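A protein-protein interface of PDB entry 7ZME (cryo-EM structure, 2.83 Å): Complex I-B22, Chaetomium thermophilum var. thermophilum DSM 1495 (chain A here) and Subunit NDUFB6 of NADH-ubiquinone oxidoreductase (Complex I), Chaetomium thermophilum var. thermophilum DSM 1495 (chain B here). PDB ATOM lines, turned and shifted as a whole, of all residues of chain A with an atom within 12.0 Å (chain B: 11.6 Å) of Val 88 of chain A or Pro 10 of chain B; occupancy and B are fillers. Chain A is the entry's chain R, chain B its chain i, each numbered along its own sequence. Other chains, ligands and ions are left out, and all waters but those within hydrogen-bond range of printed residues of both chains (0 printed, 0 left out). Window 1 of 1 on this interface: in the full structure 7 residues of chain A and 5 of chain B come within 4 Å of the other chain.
The backbone NH (N) of Glu 92 of chain A lies within hydrogen-bond range of the side-chain amide oxygen (OD1) of Asn 90 of chain A.
N of Ile 7 of chain B sits at hydrogen-bond distance from OH of Tyr 21 of chain B.
Among the printed residues, merely in contact across the chains: Leu 91 of chain A with Tyr 9 of chain B (3.4 Å), Pro 94 of chain A with His 12 of chain B (3.5 Å), Val 88 of chain A with Pro 10 of chain B (3.5 Å), Glu 92 of chain A with His 12 of chain B (3.6 Å), Leu 91 of chain A with Pro 10 of chain B (3.6 Å), Pro 93 of chain A with His 12 of chain B (3.6 Å), Pro 87 of chain A with Ile 7 of chain B (3.8 Å), Pro 87 of chain A with Pro 8 of chain B (3.8 Å) and Asn 85 of chain A with Ile 7 of chain B (3.9 Å).
Of the printed residues of chain B, Asn 85 of chain A touches Ile 7.
Pro 87 of chain A touches just these residues of chain B: Ile 7 (3.8 Å) and Pro 8 (3.8 Å).
Of chain B, only Pro 10 (3.5 Å) comes within 4 Å of Val 88 of chain A.
No residue of chain B comes within 4 Å of Pro 89 of chain A.
Leu 91 of chain A touches just these residues of chain B: Tyr 9 and Pro 10.
Of the printed residues of chain B, Glu 92 of chain A touches His 12 (3.6 Å).
Printed residues of chain B within 4 Å of Pro 93 of chain A: His 12.
Of the printed residues of chain B, Pro 94 of chain A touches His 12 (3.5 Å).
Printed residues of chain A within 4 Å of Ile 7 of chain B: Asn 85 and Pro 87.
Of chain A, only Pro 87 comes within 4 Å of Pro 8 of chain B.
Of chain A, only Leu 91 (3.4 Å) comes within 4 Å of Tyr 9 of chain B.
Of the printed residues of chain A, Pro 10 of chain B touches Val 88 and Leu 91.
No residue of chain A comes within 4 Å of Lys 11 of chain B.
Of chain A, only Glu 92 (3.6 Å), Pro 93 (3.6 Å) and Pro 94 (3.5 Å) come within 4 Å of His 12 of chain B.
Val 13 of chain B touches none of the printed residues of chain A.
The nearest residue of chain A that does not touch Pro 10 of chain B is Asn 90 of chain A (4.6 Å).
Hydrophobic or aromatic side chains of chain B within 4 Å of the printed part of chain A: Ile 7, Pro 10 and His 12.
Of the 13 printed residues of chain A, 7 touch a printed residue of chain B.
Hydrophobic or aromatic side chains of chain A that line the printed part of chain B: Pro 87, Val 88, Leu 91 and Pro 94.
Among the printed residues, no Asp or Glu carboxylate lies within 4 Å of a Lys or Arg side-chain nitrogen of the other chain.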
ATOM      1  N   GLU A  83      11.750  15.257  11.061  1.00  0.00           N
ATOM      2  CA  GLU A  83      12.305  16.271  10.155  1.00  0.00           C
ATOM      3  C   GLU A  83      12.476  17.619  10.848  1.00  0.00           C
ATOM      4  O   GLU A  83      12.415  18.677  10.223  1.00  0.00           O
ATOM      5  CB  GLU A  83      11.446  16.433   8.901  1.00  0.00           C
ATOM      6  CG  GLU A  83      11.422  15.249   7.974  1.00  0.00           C
ATOM      7  CD  GLU A  83      10.529  15.476   6.769  1.00  0.00           C
ATOM      8  OE1 GLU A  83       9.832  16.510   6.725  1.00  0.00           O
ATOM      9  OE2 GLU A  83      10.509  14.610   5.870  1.00  0.00           O
ATOM     10  N   ARG A  84      12.717  17.583  12.159  1.00  0.00           N
ATOM     11  CA  ARG A  84      12.685  18.826  12.920  1.00  0.00           C
ATOM     12  C   ARG A  84      13.940  19.662  12.697  1.00  0.00           C
ATOM     13  O   ARG A  84      13.853  20.821  12.278  1.00  0.00           O
ATOM     14  CB  ARG A  84      12.494  18.540  14.408  1.00  0.00           C
ATOM     15  CG  ARG A  84      12.761  19.747  15.282  1.00  0.00           C
ATOM     16  CD  ARG A  84      12.496  19.455  16.737  1.00  0.00           C
ATOM     17  NE  ARG A  84      11.080  19.190  16.967  1.00  0.00           N
ATOM     18  CZ  ARG A  84      10.524  19.093  18.166  1.00  0.00           C
ATOM     19  NH1 ARG A  84      11.263  19.247  19.251  1.00  0.00           N
ATOM     20  NH2 ARG A  84       9.229  18.847  18.279  1.00  0.00           N
ATOM     21  N   ASN A  85      15.112  19.093  12.959  1.00  0.00           N
ATOM     22  CA  ASN A  85      16.353  19.842  12.816  1.00  0.00           C
ATOM     23  C   ASN A  85      17.266  19.174  11.799  1.00  0.00           C
ATOM     24  O   ASN A  85      18.446  18.939  12.080  1.00  0.00           O
ATOM     25  CB  ASN A  85      17.052  19.992  14.164  1.00  0.00           C
ATOM     26  CG  ASN A  85      16.590  21.222  14.923  1.00  0.00           C
ATOM     27  OD1 ASN A  85      15.987  21.119  15.991  1.00  0.00           O
ATOM     28  ND2 ASN A  85      16.861  22.394  14.367  1.00  0.00           N
ATOM     29  N   LEU A  86      16.718  18.849  10.628  1.00  0.00           N
ATOM     30  CA  LEU A  86      17.443  18.099   9.616  1.00  0.00           C
ATOM     31  C   LEU A  86      18.770  18.778   9.284  1.00  0.00           C
ATOM     32  O   LEU A  86      18.797  19.994   9.047  1.00  0.00           O
ATOM     33  CB  LEU A  86      16.607  17.977   8.343  1.00  0.00           C
ATOM     34  CG  LEU A  86      15.522  16.909   8.257  1.00  0.00           C
ATOM     35  CD1 LEU A  86      14.640  17.172   7.050  1.00  0.00           C
ATOM     36  CD2 LEU A  86      16.138  15.530   8.180  1.00  0.00           C
ATOM     37  N   PRO A  87      19.876  18.040   9.256  1.00  0.00           N
ATOM     38  CA  PRO A  87      21.154  18.632   8.850  1.00  0.00           C
ATOM     39  C   PRO A  87      21.214  18.847   7.348  1.00  0.00           C
ATOM     40  O   PRO A  87      20.449  18.269   6.574  1.00  0.00           O
ATOM     41  CB  PRO A  87      22.181  17.592   9.300  1.00  0.00           C
ATOM     42  CG  PRO A  87      21.436  16.304   9.234  1.00  0.00           C
ATOM     43  CD  PRO A  87      20.011  16.614   9.602  1.00  0.00           C
ATOM     44  N   VAL A  88      22.147  19.702   6.940  1.00  0.00           N
ATOM     45  CA  VAL A  88      22.334  19.947   5.507  1.00  0.00           C
ATOM     46  C   VAL A  88      22.806  18.662   4.844  1.00  0.00           C
ATOM     47  O   VAL A  88      23.573  17.892   5.456  1.00  0.00           O
ATOM     48  CB  VAL A  88      23.340  21.083   5.270  1.00  0.00           C
ATOM     49  CG1 VAL A  88      22.838  22.389   5.878  1.00  0.00           C
ATOM     50  CG2 VAL A  88      24.696  20.698   5.809  1.00  0.00           C
ATOM     51  N   PRO A  89      22.372  18.359   3.621  1.00  0.00           N
ATOM     52  CA  PRO A  89      22.887  17.150   2.962  1.00  0.00           C
ATOM     53  C   PRO A  89      24.345  17.267   2.560  1.00  0.00           C
ATOM     54  O   PRO A  89      25.104  16.302   2.716  1.00  0.00           O
ATOM     55  CB  PRO A  89      21.962  17.002   1.745  1.00  0.00           C
ATOM     56  CG  PRO A  89      20.751  17.830   2.072  1.00  0.00           C
ATOM     57  CD  PRO A  89      21.261  18.969   2.877  1.00  0.00           C
ATOM     58  N   ASN A  90      24.762  18.422   2.055  1.00  0.00           N
ATOM     59  CA  ASN A  90      26.097  18.619   1.500  1.00  0.00           C
ATOM     60  C   ASN A  90      26.926  19.430   2.485  1.00  0.00           C
ATOM     61  O   ASN A  90      26.742  20.645   2.606  1.00  0.00           O
ATOM     62  CB  ASN A  90      26.004  19.327   0.149  1.00  0.00           C
ATOM     63  CG  ASN A  90      27.265  19.201  -0.668  1.00  0.00           C
ATOM     64  OD1 ASN A  90      28.346  18.966  -0.135  1.00  0.00           O
ATOM     65  ND2 ASN A  90      27.133  19.355  -1.977  1.00  0.00           N
ATOM     66  N   LEU A  91      27.840  18.765   3.188  1.00  0.00           N
ATOM     67  CA  LEU A  91      28.672  19.455   4.163  1.00  0.00           C
ATOM     68  C   LEU A  91      29.907  20.095   3.548  1.00  0.00           C
ATOM     69  O   LEU A  91      30.561  20.900   4.219  1.00  0.00           O
ATOM     70  CB  LEU A  91      29.107  18.495   5.272  1.00  0.00           C
ATOM     71  CG  LEU A  91      28.133  18.240   6.424  1.00  0.00           C
ATOM     72  CD1 LEU A  91      27.889  19.518   7.196  1.00  0.00           C
ATOM     73  CD2 LEU A  91      26.823  17.628   5.959  1.00  0.00           C
ATOM     74  N   GLU A  92      30.234  19.765   2.300  1.00  0.00           N
ATOM     75  CA  GLU A  92      31.426  20.284   1.654  1.00  0.00           C
ATOM     76  C   GLU A  92      31.237  21.742   1.241  1.00  0.00           C
ATOM     77  O   GLU A  92      30.128  22.158   0.895  1.00  0.00           O
ATOM     78  CB  GLU A  92      31.773  19.446   0.431  1.00  0.00           C
ATOM     79  CG  GLU A  92      32.610  18.213   0.739  1.00  0.00           C
ATOM     80  CD  GLU A  92      31.796  17.078   1.330  1.00  0.00           C
ATOM     81  OE1 GLU A  92      30.568  17.239   1.493  1.00  0.00           O
ATOM     82  OE2 GLU A  92      32.388  16.020   1.630  1.00  0.00           O
ATOM     83  N   PRO A  93      32.306  22.530   1.272  1.00  0.00           N
ATOM     84  CA  PRO A  93      32.212  23.936   0.871  1.00  0.00           C
ATOM     85  C   PRO A  93      31.957  24.068  -0.618  1.00  0.00           C
ATOM     86  O   PRO A  93      32.249  23.147  -1.394  1.00  0.00           O
ATOM     87  CB  PRO A  93      33.589  24.503   1.249  1.00  0.00           C
ATOM     88  CG  PRO A  93      34.164  23.529   2.215  1.00  0.00           C
ATOM     89  CD  PRO A  93      33.630  22.196   1.816  1.00  0.00           C
ATOM     90  N   PRO A  94      31.399  25.196  -1.053  1.00  0.00           N
ATOM     91  CA  PRO A  94      31.175  25.395  -2.478  1.00  0.00           C
ATOM     92  C   PRO A  94      32.487  25.412  -3.237  1.00  0.00           C
ATOM     93  O   PRO A  94      33.514  25.901  -2.732  1.00  0.00           O
ATOM     94  CB  PRO A  94      30.475  26.761  -2.540  1.00  0.00           C
ATOM     95  CG  PRO A  94      30.628  27.358  -1.189  1.00  0.00           C
ATOM     96  CD  PRO A  94      30.731  26.225  -0.245  1.00  0.00           C
ATOM     97  N   PRO A  95      32.495  24.898  -4.461  1.00  0.00           N
ATOM     98  CA  PRO A  95      33.677  25.008  -5.311  1.00  0.00           C
ATOM     99  C   PRO A  95      33.915  26.453  -5.704  1.00  0.00           C
ATOM    100  O   PRO A  95      32.977  27.262  -5.717  1.00  0.00           O
ATOM    101  CB  PRO A  95      33.308  24.155  -6.531  1.00  0.00           C
ATOM    102  CG  PRO A  95      31.828  24.235  -6.584  1.00  0.00           C
ATOM    103  CD  PRO A  95      31.374  24.247  -5.158  1.00  0.00           C
ATOM    104  N   LYS B   6      24.952  16.883  18.982  1.00  0.00           N
ATOM    105  CA  LYS B   6      25.120  18.170  18.319  1.00  0.00           C
ATOM    106  C   LYS B   6      25.026  17.949  16.818  1.00  0.00           C
ATOM    107  O   LYS B   6      25.757  17.123  16.266  1.00  0.00           O
ATOM    108  CB  LYS B   6      26.460  18.809  18.692  1.00  0.00           C
ATOM    109  CG  LYS B   6      26.528  20.298  18.445  1.00  0.00           C
ATOM    110  CD  LYS B   6      27.390  20.988  19.476  1.00  0.00           C
ATOM    111  CE  LYS B   6      26.727  20.968  20.838  1.00  0.00           C
ATOM    112  NZ  LYS B   6      27.647  21.427  21.913  1.00  0.00           N
ATOM    113  N   ILE B   7      24.132  18.680  16.170  1.00  0.00           N
ATOM    114  CA  ILE B   7      23.884  18.480  14.738  1.00  0.00           C
ATOM    115  C   ILE B   7      25.103  18.938  13.944  1.00  0.00           C
ATOM    116  O   ILE B   7      25.587  20.062  14.156  1.00  0.00           O
ATOM    117  CB  ILE B   7      22.633  19.243  14.304  1.00  0.00           C
ATOM    118  CG1 ILE B   7      21.466  18.937  15.244  1.00  0.00           C
ATOM    119  CG2 ILE B   7      22.268  18.897  12.873  1.00  0.00           C
ATOM    120  CD1 ILE B   7      21.164  17.462  15.390  1.00  0.00           C
ATOM    121  N   PRO B   8      25.634  18.122  13.038  1.00  0.00           N
ATOM    122  CA  PRO B   8      26.679  18.608  12.135  1.00  0.00           C
ATOM    123  C   PRO B   8      26.137  19.683  11.208  1.00  0.00           C
ATOM    124  O   PRO B   8      24.954  19.700  10.863  1.00  0.00           O
ATOM    125  CB  PRO B   8      27.087  17.355  11.358  1.00  0.00           C
ATOM    126  CG  PRO B   8      25.889  16.481  11.421  1.00  0.00           C
ATOM    127  CD  PRO B   8      25.291  16.717  12.771  1.00  0.00           C
ATOM    128  N   TYR B   9      27.016  20.592  10.804  1.00  0.00           N
ATOM    129  CA  TYR B   9      26.599  21.731  10.001  1.00  0.00           C
ATOM    130  C   TYR B   9      27.800  22.237   9.218  1.00  0.00           C
ATOM    131  O   TYR B   9      28.946  21.963   9.592  1.00  0.00           O
ATOM    132  CB  TYR B   9      26.023  22.845  10.883  1.00  0.00           C
ATOM    133  CG  TYR B   9      26.964  23.317  11.956  1.00  0.00           C
ATOM    134  CD1 TYR B   9      27.007  22.691  13.189  1.00  0.00           C
ATOM    135  CD2 TYR B   9      27.804  24.396  11.739  1.00  0.00           C
ATOM    136  CE1 TYR B   9      27.863  23.119  14.170  1.00  0.00           C
ATOM    137  CE2 TYR B   9      28.659  24.833  12.715  1.00  0.00           C
ATOM    138  CZ  TYR B   9      28.686  24.192  13.929  1.00  0.00           C
ATOM    139  OH  TYR B   9      29.543  24.624  14.910  1.00  0.00           O
ATOM    140  N   PRO B  10      27.574  22.965   8.125  1.00  0.00           N
ATOM    141  CA  PRO B  10      28.702  23.539   7.387  1.00  0.00           C
ATOM    142  C   PRO B  10      29.372  24.643   8.181  1.00  0.00           C
ATOM    143  O   PRO B  10      28.712  25.474   8.806  1.00  0.00           O
ATOM    144  CB  PRO B  10      28.055  24.095   6.112  1.00  0.00           C
ATOM    145  CG  PRO B  10      26.657  23.580   6.100  1.00  0.00           C
ATOM    146  CD  PRO B  10      26.285  23.320   7.513  1.00  0.00           C
ATOM    147  N   LYS B  11      30.697  24.653   8.143  1.00  0.00           N
ATOM    148  CA  LYS B  11      31.472  25.718   8.755  1.00  0.00           C
ATOM    149  C   LYS B  11      31.713  26.878   7.802  1.00  0.00           C
ATOM    150  O   LYS B  11      32.390  27.840   8.174  1.00  0.00           O
ATOM    151  CB  LYS B  11      32.809  25.170   9.258  1.00  0.00           C
ATOM    152  CG  LYS B  11      32.681  23.894  10.067  1.00  0.00           C
ATOM    153  CD  LYS B  11      31.993  24.153  11.392  1.00  0.00           C
ATOM    154  CE  LYS B  11      31.509  22.859  12.020  1.00  0.00           C
ATOM    155  NZ  LYS B  11      30.657  22.073  11.086  1.00  0.00           N
ATOM    156  N   HIS B  12      31.178  26.805   6.587  1.00  0.00           N
ATOM    157  CA  HIS B  12      31.372  27.824   5.571  1.00  0.00           C
ATOM    158  C   HIS B  12      30.186  28.766   5.438  1.00  0.00           C
ATOM    159  O   HIS B  12      30.220  29.665   4.593  1.00  0.00           O
ATOM    160  CB  HIS B  12      31.667  27.164   4.220  1.00  0.00           C
ATOM    161  CG  HIS B  12      30.474  26.525   3.579  1.00  0.00           C
ATOM    162  ND1 HIS B  12      30.243  25.168   3.626  1.00  0.00           N
ATOM    163  CD2 HIS B  12      29.457  27.053   2.857  1.00  0.00           C
ATOM    164  CE1 HIS B  12      29.130  24.889   2.970  1.00  0.00           C
ATOM    165  NE2 HIS B  12      28.634  26.016   2.495  1.00  0.00           N
ATOM    166  N   VAL B  13      29.149  28.597   6.253  1.00  0.00           N
ATOM    167  CA  VAL B  13      27.926  29.382   6.147  1.00  0.00           C
ATOM    168  C   VAL B  13      27.970  30.490   7.190  1.00  0.00           C
ATOM    169  O   VAL B  13      28.136  30.225   8.386  1.00  0.00           O
ATOM    170  CB  VAL B  13      26.681  28.501   6.323  1.00  0.00           C
ATOM    171  CG1 VAL B  13      25.443  29.354   6.485  1.00  0.00           C
ATOM    172  CG2 VAL B  13      26.532  27.560   5.142  1.00  0.00           C
ATOM    173  N   TRP B  14      27.822  31.731   6.736  1.00  0.00           N
ATOM    174  CA  TRP B  14      27.881  32.908   7.591  1.00  0.00           C
ATOM    175  C   TRP B  14      26.464  33.385   7.885  1.00  0.00           C
ATOM    176  O   TRP B  14      25.707  33.701   6.962  1.00  0.00           O
ATOM    177  CB  TRP B  14      28.689  34.020   6.922  1.00  0.00           C
ATOM    178  CG  TRP B  14      29.131  35.108   7.851  1.00  0.00           C
ATOM    179  CD1 TRP B  14      30.329  35.200   8.482  1.00  0.00           C
ATOM    180  CD2 TRP B  14      28.380  36.264   8.244  1.00  0.00           C
ATOM    181  NE1 TRP B  14      30.376  36.335   9.250  1.00  0.00           N
ATOM    182  CE2 TRP B  14      29.190  37.006   9.120  1.00  0.00           C
ATOM    183  CE3 TRP B  14      27.102  36.741   7.941  1.00  0.00           C
ATOM    184  CZ2 TRP B  14      28.767  38.200   9.697  1.00  0.00           C
ATOM    185  CZ3 TRP B  14      26.682  37.925   8.517  1.00  0.00           C
ATOM    186  CH2 TRP B  14      27.510  38.639   9.385  1.00  0.00           C
ATOM    187  N   SER B  15      26.115  33.450   9.164  1.00  0.00           N
ATOM    188  CA  SER B  15      24.802  33.899   9.571  1.00  0.00           C
ATOM    189  C   SER B  15      24.918  35.129  10.461  1.00  0.00           C
ATOM    190  O   SER B  15      25.845  35.219  11.270  1.00  0.00           O
ATOM    191  CB  SER B  15      24.055  32.790  10.324  1.00  0.00           C
ATOM    192  OG  SER B  15      22.781  33.224  10.754  1.00  0.00           O
ATOM    193  N   GLY B  18      24.149  34.208  13.982  1.00  0.00           N
ATOM    194  CA  GLY B  18      25.196  33.429  14.604  1.00  0.00           C
ATOM    195  C   GLY B  18      25.535  32.127  13.916  1.00  0.00           C
ATOM    196  O   GLY B  18      26.714  31.812  13.727  1.00  0.00           O
ATOM    197  N   GLY B  19      24.526  31.369  13.513  1.00  0.00           N
ATOM    198  CA  GLY B  19      24.793  30.076  12.923  1.00  0.00           C
ATOM    199  C   GLY B  19      24.141  28.943  13.680  1.00  0.00           C
ATOM    200  O   GLY B  19      22.937  28.980  13.935  1.00  0.00           O
ATOM    201  N   TRP B  20      24.915  27.923  14.048  1.00  0.00           N
ATOM    202  CA  TRP B  20      24.340  26.737  14.668  1.00  0.00           C
ATOM    203  C   TRP B  20      24.492  26.720  16.184  1.00  0.00           C
ATOM    204  O   TRP B  20      23.492  26.680  16.896  1.00  0.00           O
ATOM    205  CB  TRP B  20      24.928  25.473  14.039  1.00  0.00           C
ATOM    206  CG  TRP B  20      24.150  25.049  12.847  1.00  0.00           C
ATOM    207  CD1 TRP B  20      23.177  24.099  12.807  1.00  0.00           C
ATOM    208  CD2 TRP B  20      24.237  25.593  11.528  1.00  0.00           C
ATOM    209  NE1 TRP B  20      22.668  23.994  11.539  1.00  0.00           N
ATOM    210  CE2 TRP B  20      23.301  24.904  10.734  1.00  0.00           C
ATOM    211  CE3 TRP B  20      25.027  26.579  10.937  1.00  0.00           C
ATOM    212  CZ2 TRP B  20      23.136  25.171   9.384  1.00  0.00           C
ATOM    213  CZ3 TRP B  20      24.859  26.845   9.599  1.00  0.00           C
ATOM    214  CH2 TRP B  20      23.922  26.143   8.835  1.00  0.00           C
ATOM    215  N   TYR B  21      25.706  26.766  16.701  1.00  0.00           N
ATOM    216  CA  TYR B  21      25.862  26.820  18.149  1.00  0.00           C
ATOM    217  C   TYR B  21      26.777  27.963  18.522  1.00  0.00           C
ATOM    218  O   TYR B  21      27.652  27.837  19.381  1.00  0.00           O
ATOM    219  CB  TYR B  21      26.369  25.489  18.698  1.00  0.00           C
ATOM    220  CG  TYR B  21      25.388  24.353  18.512  1.00  0.00           C
ATOM    221  CD1 TYR B  21      25.335  23.644  17.320  1.00  0.00           C
ATOM    222  CD2 TYR B  21      24.505  23.999  19.521  1.00  0.00           C
ATOM    223  CE1 TYR B  21      24.436  22.616  17.142  1.00  0.00           C
ATOM    224  CE2 TYR B  21      23.606  22.970  19.352  1.00  0.00           C
ATOM    225  CZ  TYR B  21      23.576  22.282  18.162  1.00  0.00           C
ATOM    226  OH  TYR B  21      22.678  21.254  17.992  1.00  0.00           O
ATOM    227  N   ALA B  22      26.556  29.112  17.891  1.00  0.00           N
ATOM    228  CA  ALA B  22      27.539  30.185  17.854  1.00  0.00           C
ATOM    229  C   ALA B  22      27.576  30.925  19.184  1.00  0.00           C
ATOM    230  O   ALA B  22      26.601  31.572  19.576  1.00  0.00           O
ATOM    231  CB  ALA B  22      27.224  31.140  16.710  1.00  0.00           C
